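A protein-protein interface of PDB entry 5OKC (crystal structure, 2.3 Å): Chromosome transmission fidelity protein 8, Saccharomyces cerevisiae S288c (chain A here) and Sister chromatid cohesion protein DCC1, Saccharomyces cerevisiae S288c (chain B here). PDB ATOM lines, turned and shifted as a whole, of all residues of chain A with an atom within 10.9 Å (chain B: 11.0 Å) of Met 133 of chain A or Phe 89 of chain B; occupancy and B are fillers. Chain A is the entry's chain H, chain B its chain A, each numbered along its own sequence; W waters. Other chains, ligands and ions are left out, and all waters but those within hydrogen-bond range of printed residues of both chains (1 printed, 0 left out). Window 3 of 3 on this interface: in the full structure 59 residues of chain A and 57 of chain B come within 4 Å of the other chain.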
ATOM      1  N   SER A  72       4.819 -23.024   4.640  1.00  0.00           N
ATOM      2  CA  SER A  72       3.613 -22.543   5.303  1.00  0.00           C
ATOM      3  C   SER A  72       3.187 -21.207   4.712  1.00  0.00           C
ATOM      4  O   SER A  72       4.025 -20.392   4.336  1.00  0.00           O
ATOM      5  CB  SER A  72       3.839 -22.402   6.810  1.00  0.00           C
ATOM      6  OG  SER A  72       4.223 -23.633   7.394  1.00  0.00           O
ATOM      7  N   LEU A  73       1.881 -20.987   4.629  1.00  0.00           N
ATOM      8  CA  LEU A  73       1.364 -19.741   4.081  1.00  0.00           C
ATOM      9  C   LEU A  73       0.458 -19.031   5.076  1.00  0.00           C
ATOM     10  O   LEU A  73      -0.432 -19.641   5.664  1.00  0.00           O
ATOM     11  CB  LEU A  73       0.611 -20.004   2.776  1.00  0.00           C
ATOM     12  CG  LEU A  73       0.012 -18.776   2.091  1.00  0.00           C
ATOM     13  CD1 LEU A  73       1.105 -17.786   1.723  1.00  0.00           C
ATOM     14  CD2 LEU A  73      -0.774 -19.185   0.859  1.00  0.00           C
ATOM     15  N   GLN A  74       0.694 -17.737   5.259  1.00  0.00           N
ATOM     16  CA  GLN A  74      -0.083 -16.938   6.194  1.00  0.00           C
ATOM     17  C   GLN A  74      -0.663 -15.720   5.487  1.00  0.00           C
ATOM     18  O   GLN A  74       0.078 -14.868   4.998  1.00  0.00           O
ATOM     19  CB  GLN A  74       0.779 -16.506   7.380  1.00  0.00           C
ATOM     20  CG  GLN A  74       0.053 -15.633   8.390  1.00  0.00           C
ATOM     21  CD  GLN A  74      -0.708 -16.445   9.417  1.00  0.00           C
ATOM     22  OE1 GLN A  74      -0.222 -17.467   9.902  1.00  0.00           O
ATOM     23  NE2 GLN A  74      -1.911 -15.995   9.753  1.00  0.00           N
ATOM     24  N   ILE A  75      -1.988 -15.641   5.433  1.00  0.00           N
ATOM     25  CA  ILE A  75      -2.653 -14.549   4.732  1.00  0.00           C
ATOM     26  C   ILE A  75      -3.225 -13.511   5.692  1.00  0.00           C
ATOM     27  O   ILE A  75      -4.111 -13.808   6.494  1.00  0.00           O
ATOM     28  CB  ILE A  75      -3.788 -15.071   3.833  1.00  0.00           C
ATOM     29  CG1 ILE A  75      -3.272 -16.187   2.921  1.00  0.00           C
ATOM     30  CG2 ILE A  75      -4.380 -13.936   3.015  1.00  0.00           C
ATOM     31  CD1 ILE A  75      -2.134 -15.759   2.022  1.00  0.00           C
ATOM     32  N   ALA A  80       0.727 -11.198   2.427  1.00  0.00           N
ATOM     33  CA  ALA A  80       0.929 -12.633   2.560  1.00  0.00           C
ATOM     34  C   ALA A  80       2.367 -12.932   2.956  1.00  0.00           C
ATOM     35  O   ALA A  80       3.296 -12.242   2.534  1.00  0.00           O
ATOM     36  CB  ALA A  80       0.575 -13.344   1.263  1.00  0.00           C
ATOM     37  N   THR A  81       2.544 -13.968   3.769  1.00  0.00           N
ATOM     38  CA  THR A  81       3.876 -14.383   4.180  1.00  0.00           C
ATOM     39  C   THR A  81       4.064 -15.870   3.919  1.00  0.00           C
ATOM     40  O   THR A  81       3.202 -16.688   4.243  1.00  0.00           O
ATOM     41  CB  THR A  81       4.128 -14.088   5.673  1.00  0.00           C
ATOM     42  OG1 THR A  81       3.823 -12.716   5.952  1.00  0.00           O
ATOM     43  CG2 THR A  81       5.580 -14.366   6.035  1.00  0.00           C
ATOM     44  N   LEU A  82       5.201 -16.208   3.325  1.00  0.00           N
ATOM     45  CA  LEU A  82       5.495 -17.583   2.960  1.00  0.00           C
ATOM     46  C   LEU A  82       6.752 -18.087   3.647  1.00  0.00           C
ATOM     47  O   LEU A  82       7.823 -17.523   3.477  1.00  0.00           O
ATOM     48  CB  LEU A  82       5.646 -17.707   1.444  1.00  0.00           C
ATOM     49  CG  LEU A  82       6.262 -19.001   0.918  1.00  0.00           C
ATOM     50  CD1 LEU A  82       5.382 -20.179   1.274  1.00  0.00           C
ATOM     51  CD2 LEU A  82       6.473 -18.923  -0.583  1.00  0.00           C
ATOM     52  N   PHE A  83       6.621 -19.152   4.424  1.00  0.00           N
ATOM     53  CA  PHE A  83       7.788 -19.790   5.006  1.00  0.00           C
ATOM     54  C   PHE A  83       8.181 -20.970   4.137  1.00  0.00           C
ATOM     55  O   PHE A  83       7.348 -21.814   3.819  1.00  0.00           O
ATOM     56  CB  PHE A  83       7.510 -20.236   6.441  1.00  0.00           C
ATOM     57  CG  PHE A  83       7.270 -19.099   7.388  1.00  0.00           C
ATOM     58  CD1 PHE A  83       5.996 -18.585   7.565  1.00  0.00           C
ATOM     59  CD2 PHE A  83       8.318 -18.541   8.100  1.00  0.00           C
ATOM     60  CE1 PHE A  83       5.772 -17.536   8.438  1.00  0.00           C
ATOM     61  CE2 PHE A  83       8.101 -17.492   8.973  1.00  0.00           C
ATOM     62  CZ  PHE A  83       6.826 -16.990   9.142  1.00  0.00           C
ATOM     63  N   VAL A  84       9.447 -21.011   3.737  1.00  0.00           N
ATOM     64  CA  VAL A  84       9.954 -22.097   2.911  1.00  0.00           C
ATOM     65  C   VAL A  84      11.082 -22.829   3.625  1.00  0.00           C
ATOM     66  O   VAL A  84      12.051 -22.212   4.094  1.00  0.00           O
ATOM     67  CB  VAL A  84      10.461 -21.592   1.546  1.00  0.00           C
ATOM     68  CG1 VAL A  84      11.034 -22.743   0.733  1.00  0.00           C
ATOM     69  CG2 VAL A  84       9.341 -20.908   0.783  1.00  0.00           C
ATOM     70  N   LYS A  86      13.147 -24.646   6.413  1.00  0.00           N
ATOM     71  CA  LYS A  86      13.341 -24.304   7.811  1.00  0.00           C
ATOM     72  C   LYS A  86      13.952 -22.916   7.936  1.00  0.00           C
ATOM     73  O   LYS A  86      13.971 -22.334   9.019  1.00  0.00           O
ATOM     74  CB  LYS A  86      14.238 -25.336   8.497  1.00  0.00           C
ATOM     75  CG  LYS A  86      13.720 -26.762   8.416  1.00  0.00           C
ATOM     76  CD  LYS A  86      14.758 -27.750   8.919  1.00  0.00           C
ATOM     77  CE  LYS A  86      16.022 -27.692   8.074  1.00  0.00           C
ATOM     78  NZ  LYS A  86      16.998 -28.755   8.444  1.00  0.00           N
ATOM     79  N   LYS A  87      14.449 -22.386   6.822  1.00  0.00           N
ATOM     80  CA  LYS A  87      15.309 -21.211   6.884  1.00  0.00           C
ATOM     81  C   LYS A  87      14.897 -20.032   6.005  1.00  0.00           C
ATOM     82  O   LYS A  87      15.618 -19.035   5.953  1.00  0.00           O
ATOM     83  CB  LYS A  87      16.742 -21.614   6.522  1.00  0.00           C
ATOM     84  CG  LYS A  87      17.307 -22.726   7.390  1.00  0.00           C
ATOM     85  CD  LYS A  87      18.622 -23.247   6.837  1.00  0.00           C
ATOM     86  CE  LYS A  87      19.132 -24.426   7.651  1.00  0.00           C
ATOM     87  NZ  LYS A  87      20.346 -25.037   7.041  1.00  0.00           N
ATOM     88  N   GLN A  88      13.761 -20.117   5.317  1.00  0.00           N
ATOM     89  CA  GLN A  88      13.396 -19.007   4.439  1.00  0.00           C
ATOM     90  C   GLN A  88      12.047 -18.371   4.750  1.00  0.00           C
ATOM     91  O   GLN A  88      11.081 -19.052   5.095  1.00  0.00           O
ATOM     92  CB  GLN A  88      13.420 -19.452   2.977  1.00  0.00           C
ATOM     93  CG  GLN A  88      14.822 -19.621   2.419  1.00  0.00           C
ATOM     94  CD  GLN A  88      14.828 -19.802   0.914  1.00  0.00           C
ATOM     95  OE1 GLN A  88      13.887 -20.347   0.338  1.00  0.00           O
ATOM     96  NE2 GLN A  88      15.891 -19.338   0.268  1.00  0.00           N
ATOM     97  N   ARG A  89      12.002 -17.049   4.624  1.00  0.00           N
ATOM     98  CA  ARG A  89      10.772 -16.282   4.765  1.00  0.00           C
ATOM     99  C   ARG A  89      10.648 -15.264   3.631  1.00  0.00           C
ATOM    100  O   ARG A  89      11.550 -14.458   3.403  1.00  0.00           O
ATOM    101  CB  ARG A  89      10.735 -15.584   6.128  1.00  0.00           C
ATOM    102  CG  ARG A  89       9.538 -14.673   6.343  1.00  0.00           C
ATOM    103  CD  ARG A  89       9.510 -14.138   7.769  1.00  0.00           C
ATOM    104  NE  ARG A  89      10.750 -13.455   8.126  1.00  0.00           N
ATOM    105  CZ  ARG A  89      10.893 -12.134   8.168  1.00  0.00           C
ATOM    106  NH1 ARG A  89       9.867 -11.344   7.882  1.00  0.00           N
ATOM    107  NH2 ARG A  89      12.061 -11.603   8.502  1.00  0.00           N
ATOM    108  N   LEU A  90       9.522 -15.309   2.928  1.00  0.00           N
ATOM    109  CA  LEU A  90       9.273 -14.442   1.785  1.00  0.00           C
ATOM    110  C   LEU A  90       8.025 -13.601   2.006  1.00  0.00           C
ATOM    111  O   LEU A  90       6.990 -14.114   2.429  1.00  0.00           O
ATOM    112  CB  LEU A  90       9.118 -15.264   0.501  1.00  0.00           C
ATOM    113  CG  LEU A  90      10.319 -16.043  -0.046  1.00  0.00           C
ATOM    114  CD1 LEU A  90      10.528 -17.352   0.700  1.00  0.00           C
ATOM    115  CD2 LEU A  90      10.143 -16.302  -1.533  1.00  0.00           C
ATOM    116  N   LEU A  91       8.123 -12.310   1.717  1.00  0.00           N
ATOM    117  CA  LEU A  91       6.977 -11.419   1.839  1.00  0.00           C
ATOM    118  C   LEU A  91       6.348 -11.175   0.471  1.00  0.00           C
ATOM    119  O   LEU A  91       7.046 -10.864  -0.495  1.00  0.00           O
ATOM    120  CB  LEU A  91       7.390 -10.095   2.481  1.00  0.00           C
ATOM    121  CG  LEU A  91       8.040 -10.208   3.862  1.00  0.00           C
ATOM    122  CD1 LEU A  91       8.381  -8.831   4.412  1.00  0.00           C
ATOM    123  CD2 LEU A  91       7.140 -10.970   4.824  1.00  0.00           C
ATOM    124  N   PRO A 129      13.981 -13.648  -0.626  1.00  0.00           N
ATOM    125  CA  PRO A 129      13.723 -14.347   0.639  1.00  0.00           C
ATOM    126  C   PRO A 129      14.502 -13.760   1.813  1.00  0.00           C
ATOM    127  O   PRO A 129      15.631 -13.306   1.641  1.00  0.00           O
ATOM    128  CB  PRO A 129      14.189 -15.777   0.348  1.00  0.00           C
ATOM    129  CG  PRO A 129      14.055 -15.923  -1.121  1.00  0.00           C
ATOM    130  CD  PRO A 129      14.395 -14.579  -1.691  1.00  0.00           C
ATOM    131  N   LEU A 130      13.892 -13.768   2.993  1.00  0.00           N
ATOM    132  CA  LEU A 130      14.522 -13.228   4.189  1.00  0.00           C
ATOM    133  C   LEU A 130      14.803 -14.342   5.190  1.00  0.00           C
ATOM    134  O   LEU A 130      14.238 -15.430   5.079  1.00  0.00           O
ATOM    135  CB  LEU A 130      13.629 -12.159   4.829  1.00  0.00           C
ATOM    136  CG  LEU A 130      13.284 -10.927   3.993  1.00  0.00           C
ATOM    137  CD1 LEU A 130      12.303 -10.040   4.741  1.00  0.00           C
ATOM    138  CD2 LEU A 130      14.546 -10.154   3.641  1.00  0.00           C
ATOM    139  N   PRO A 131      15.684 -14.075   6.168  1.00  0.00           N
ATOM    140  CA  PRO A 131      15.832 -14.967   7.324  1.00  0.00           C
ATOM    141  C   PRO A 131      14.512 -15.143   8.071  1.00  0.00           C
ATOM    142  O   PRO A 131      13.620 -14.304   7.941  1.00  0.00           O
ATOM    143  CB  PRO A 131      16.864 -14.246   8.192  1.00  0.00           C
ATOM    144  CG  PRO A 131      17.668 -13.453   7.225  1.00  0.00           C
ATOM    145  CD  PRO A 131      16.707 -13.015   6.159  1.00  0.00           C
ATOM    146  N   ILE A 132      14.388 -16.221   8.838  1.00  0.00           N
ATOM    147  CA  ILE A 132      13.129 -16.549   9.501  1.00  0.00           C
ATOM    148  C   ILE A 132      12.722 -15.511  10.552  1.00  0.00           C
ATOM    149  O   ILE A 132      11.583 -15.506  11.019  1.00  0.00           O
ATOM    150  CB  ILE A 132      13.196 -17.937  10.165  1.00  0.00           C
ATOM    151  CG1 ILE A 132      14.373 -18.009  11.140  1.00  0.00           C
ATOM    152  CG2 ILE A 132      13.318 -19.023   9.111  1.00  0.00           C
ATOM    153  CD1 ILE A 132      14.504 -19.346  11.836  1.00  0.00           C
ATOM    154  N   MET A 133      13.653 -14.633  10.916  1.00  0.00           N
ATOM    155  CA  MET A 133      13.360 -13.546  11.845  1.00  0.00           C
ATOM    156  C   MET A 133      14.414 -12.447  11.750  1.00  0.00           C
ATOM    157  O   MET A 133      14.185 -11.312  12.167  1.00  0.00           O
ATOM    158  OXT MET A 133      15.518 -12.668  11.252  1.00  0.00           O
ATOM    159  CB  MET A 133      13.272 -14.069  13.280  1.00  0.00           C
ATOM    160  CG  MET A 133      14.596 -14.534  13.856  1.00  0.00           C
ATOM    161  SD  MET A 133      14.357 -15.586  15.478  1.00  0.00           S
ATOM    162  CE  MET A 133      13.548 -17.165  14.675  1.00  0.00           C
ATOM    163  N   SER B   2      -2.377 -20.576   9.742  1.00  0.00           N
ATOM    164  CA  SER B   2      -1.532 -20.729   8.561  1.00  0.00           C
ATOM    165  C   SER B   2      -2.007 -21.879   7.685  1.00  0.00           C
ATOM    166  O   SER B   2      -2.846 -22.683   8.093  1.00  0.00           O
ATOM    167  CB  SER B   2      -0.075 -20.955   8.967  1.00  0.00           C
ATOM    168  OG  SER B   2       0.070 -22.193   9.638  1.00  0.00           O
ATOM    169  N   PHE B  83       4.067 -31.783  13.142  1.00  0.00           N
ATOM    170  CA  PHE B  83       5.484 -31.452  13.105  1.00  0.00           C
ATOM    171  C   PHE B  83       5.837 -30.532  14.270  1.00  0.00           C
ATOM    172  O   PHE B  83       5.006 -29.748  14.730  1.00  0.00           O
ATOM    173  CB  PHE B  83       5.871 -30.808  11.769  1.00  0.00           C
ATOM    174  CG  PHE B  83       5.086 -29.571  11.428  1.00  0.00           C
ATOM    175  CD1 PHE B  83       5.528 -28.319  11.829  1.00  0.00           C
ATOM    176  CD2 PHE B  83       3.917 -29.658  10.688  1.00  0.00           C
ATOM    177  CE1 PHE B  83       4.811 -27.181  11.508  1.00  0.00           C
ATOM    178  CE2 PHE B  83       3.197 -28.524  10.364  1.00  0.00           C
ATOM    179  CZ  PHE B  83       3.645 -27.283  10.775  1.00  0.00           C
ATOM    180  N   GLU B  85       6.953 -27.535  16.293  1.00  0.00           N
ATOM    181  CA  GLU B  85       6.925 -26.096  16.090  1.00  0.00           C
ATOM    182  C   GLU B  85       8.148 -25.424  16.699  1.00  0.00           C
ATOM    183  O   GLU B  85       8.465 -25.619  17.872  1.00  0.00           O
ATOM    184  CB  GLU B  85       5.648 -25.513  16.703  1.00  0.00           C
ATOM    185  CG  GLU B  85       5.517 -24.003  16.605  1.00  0.00           C
ATOM    186  CD  GLU B  85       5.515 -23.496  15.178  1.00  0.00           C
ATOM    187  OE1 GLU B  85       5.089 -24.243  14.270  1.00  0.00           O
ATOM    188  OE2 GLU B  85       5.933 -22.341  14.966  1.00  0.00           O
ATOM    189  N   THR B  86       8.831 -24.633  15.879  1.00  0.00           N
ATOM    190  CA  THR B  86      10.034 -23.933  16.306  1.00  0.00           C
ATOM    191  C   THR B  86       9.730 -22.450  16.486  1.00  0.00           C
ATOM    192  O   THR B  86       8.571 -22.060  16.635  1.00  0.00           O
ATOM    193  CB  THR B  86      11.186 -24.112  15.296  1.00  0.00           C
ATOM    194  OG1 THR B  86      10.918 -25.242  14.455  1.00  0.00           O
ATOM    195  CG2 THR B  86      12.512 -24.325  16.021  1.00  0.00           C
ATOM    196  N   LEU B  87      10.773 -21.627  16.477  1.00  0.00           N
ATOM    197  CA  LEU B  87      10.610 -20.185  16.612  1.00  0.00           C
ATOM    198  C   LEU B  87      10.044 -19.554  15.340  1.00  0.00           C
ATOM    199  O   LEU B  87      10.744 -18.827  14.637  1.00  0.00           O
ATOM    200  CB  LEU B  87      11.947 -19.525  16.967  1.00  0.00           C
ATOM    201  CG  LEU B  87      12.675 -19.984  18.234  1.00  0.00           C
ATOM    202  CD1 LEU B  87      11.688 -20.304  19.351  1.00  0.00           C
ATOM    203  CD2 LEU B  87      13.600 -21.166  17.959  1.00  0.00           C
ATOM    204  N   LEU B  88       8.780 -19.837  15.044  1.00  0.00           N
ATOM    205  CA  LEU B  88       8.149 -19.295  13.848  1.00  0.00           C
ATOM    206  C   LEU B  88       7.191 -18.164  14.206  1.00  0.00           C
ATOM    207  O   LEU B  88       6.156 -18.386  14.832  1.00  0.00           O
ATOM    208  CB  LEU B  88       7.415 -20.392  13.075  1.00  0.00           C
ATOM    209  CG  LEU B  88       8.270 -21.584  12.638  1.00  0.00           C
ATOM    210  CD1 LEU B  88       7.427 -22.615  11.901  1.00  0.00           C
ATOM    211  CD2 LEU B  88       9.432 -21.120  11.773  1.00  0.00           C
ATOM    212  N   PHE B  89       7.546 -16.954  13.792  1.00  0.00           N
ATOM    213  CA  PHE B  89       6.805 -15.753  14.158  1.00  0.00           C
ATOM    214  C   PHE B  89       6.098 -15.196  12.934  1.00  0.00           C
ATOM    215  O   PHE B  89       6.661 -15.175  11.840  1.00  0.00           O
ATOM    216  CB  PHE B  89       7.731 -14.704  14.773  1.00  0.00           C
ATOM    217  CG  PHE B  89       8.623 -15.244  15.853  1.00  0.00           C
ATOM    218  CD1 PHE B  89       8.157 -15.371  17.151  1.00  0.00           C
ATOM    219  CD2 PHE B  89       9.925 -15.627  15.574  1.00  0.00           C
ATOM    220  CE1 PHE B  89       8.971 -15.865  18.150  1.00  0.00           C
ATOM    221  CE2 PHE B  89      10.744 -16.122  16.570  1.00  0.00           C
ATOM    222  CZ  PHE B  89      10.266 -16.242  17.859  1.00  0.00           C
ATOM    223  N   GLY B  90       4.863 -14.745  13.119  1.00  0.00           N
ATOM    224  CA  GLY B  90       4.064 -14.285  12.002  1.00  0.00           C
ATOM    225  C   GLY B  90       3.366 -15.494  11.414  1.00  0.00           C
ATOM    226  O   GLY B  90       2.826 -15.451  10.308  1.00  0.00           O
ATOM    227  N   LEU B  91       3.387 -16.583  12.177  1.00  0.00           N
ATOM    228  CA  LEU B  91       2.811 -17.848  11.745  1.00  0.00           C
ATOM    229  C   LEU B  91       1.827 -18.375  12.782  1.00  0.00           C
ATOM    230  O   LEU B  91       2.207 -18.725  13.901  1.00  0.00           O
ATOM    231  CB  LEU B  91       3.917 -18.878  11.490  1.00  0.00           C
ATOM    232  CG  LEU B  91       3.521 -20.268  10.984  1.00  0.00           C
ATOM    233  CD1 LEU B  91       4.546 -20.760   9.982  1.00  0.00           C
ATOM    234  CD2 LEU B  91       3.389 -21.267  12.130  1.00  0.00           C
ATOM    235  N   SER B  92       0.559 -18.425  12.394  1.00  0.00           N
ATOM    236  CA  SER B  92      -0.493 -18.971  13.240  1.00  0.00           C
ATOM    237  C   SER B  92      -0.596 -20.479  13.048  1.00  0.00           C
ATOM    238  O   SER B  92       0.039 -21.043  12.157  1.00  0.00           O
ATOM    239  CB  SER B  92      -1.836 -18.300  12.940  1.00  0.00           C
ATOM    240  OG  SER B  92      -2.214 -18.491  11.588  1.00  0.00           O
ATOM    241  N   LYS B  93      -1.385 -21.123  13.900  1.00  0.00           N
ATOM    242  CA  LYS B  93      -1.574 -22.568  13.863  1.00  0.00           C
ATOM    243  C   LYS B  93      -2.101 -22.996  12.493  1.00  0.00           C
ATOM    244  O   LYS B  93      -2.970 -22.330  11.929  1.00  0.00           O
ATOM    245  CB  LYS B  93      -2.547 -22.993  14.964  1.00  0.00           C
ATOM    246  CG  LYS B  93      -2.479 -24.453  15.364  1.00  0.00           C
ATOM    247  CD  LYS B  93      -1.196 -24.722  16.138  1.00  0.00           C
ATOM    248  CE  LYS B  93      -1.174 -26.121  16.732  1.00  0.00           C
ATOM    249  NZ  LYS B  93       0.111 -26.396  17.437  1.00  0.00           N
HETATM  250  O   HOH W   1       9.287 -13.604  11.336  1.00  0.00           O
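Of the printed residues of chain B, Met 133 of chain A touches Leu 87 and Phe 89.
Phe 89 of chain B touches two residues of chain A.
No residue of chain B comes within 4 Å of Pro 131 of chain A.
Of chain A, only Met 133 comes within 4 Å of Leu 87 of chain B.
No residue of chain A comes within 4 Å of Leu 88 of chain B.
Gly 90 of chain B touches just one residue of chain A: Gln 74.
Leu 91 of chain B touches just these residues of chain A: Ser 72 (3.6 Å), Gln 74 (3.6 Å) and Phe 83 (3.6 Å).
Of the printed residues of chain B, Gln 74 of chain A touches Ser 2 (3.6 Å), Gly 90 (3.4 Å), Leu 91 (3.6 Å) and Ser 92 (2.8 Å).
Of the printed residues of chain B, Ser 72 of chain A touches Leu 91 (3.6 Å).
Of the printed residues of chain A, Ser 92 of chain B touches Gln 74.
Printed residues of chain A within 4 Å of Ser 2 of chain B: Leu 73 and Gln 74.
Of the printed residues of chain B, Leu 73 of chain A touches Ser 2.
Thr 86 of chain B touches none of the printed residues of chain A.
Val 84 of chain A touches none of the printed residues of chain B.
The nearest residue of chain B that does not touch Met 133 of chain A is Leu 88 of chain B (5.5 Å).
The nearest residue of chain A that does not touch Phe 89 of chain B is Ile 132 of chain A (4.8 Å).
The nearest printed residue of chain B that does not touch Gln 74 of chain A is Lys 93 of chain B (5.5 Å).
The backbone NH of Thr 81 of chain A is in hydrogen-bond range of the backbone carbonyl oxygen of Gln 74 of chain A (2.9 Å).
N of Ser 2 of chain B is in hydrogen-bond range of O of Lys 93 of chain B.
OG of Ser 2 of chain B is in hydrogen-bond range of O of Ser 92 of chain B (2.8 Å).
The backbone carbonyl oxygen of Ser 72 of chain A sits at hydrogen-bond distance from the backbone NH of Phe 83 of chain A (2.9 Å).
Water W1 bridges the backbone carbonyl oxygen of Ile 132 of chain A (3.0 Å) and the backbone carbonyl oxygen of Phe 89 of chain B (3.1 Å).
Hydrophobic or aromatic side chains of chain B that line the printed part of chain A: Leu 87, Phe 89 and Leu 91.
Printed residues of chain A that touch a printed residue of chain B: Ser 72, Leu 73, Gln 74, Phe 83 and Met 133.
Among the printed residues, 10 pairs touch across the chains.
Among the printed residues, no Asp or Glu carboxylate lies within 4 Å of a Lys or Arg side-chain nitrogen of the other chain.
N of Ser 92 of chain B sits at hydrogen-bond distance from OE1 of Gln 74 of chain A (2.8 Å).
Among the printed residues, merely in contact across the chains: Phe 83 of chain A with Phe 89 of chain B (3.3 Å), Met 133 of chain A with Leu 87 of chain B (3.3 Å), Leu 73 of chain A with Ser 2 of chain B (3.3 Å), Gln 74 of chain A with Gly 90 of chain B (3.4 Å), Met 133 of chain A with Phe 89 of chain B (3.5 Å), Phe 83 of chain A with Leu 91 of chain B (3.6 Å), Gln 74 of chain A with Leu 91 of chain B (3.6 Å), Gln 74 of chain A with Ser 2 of chain B (3.6 Å) and Ser 72 of chain A with Leu 91 of chain B (3.6 Å).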
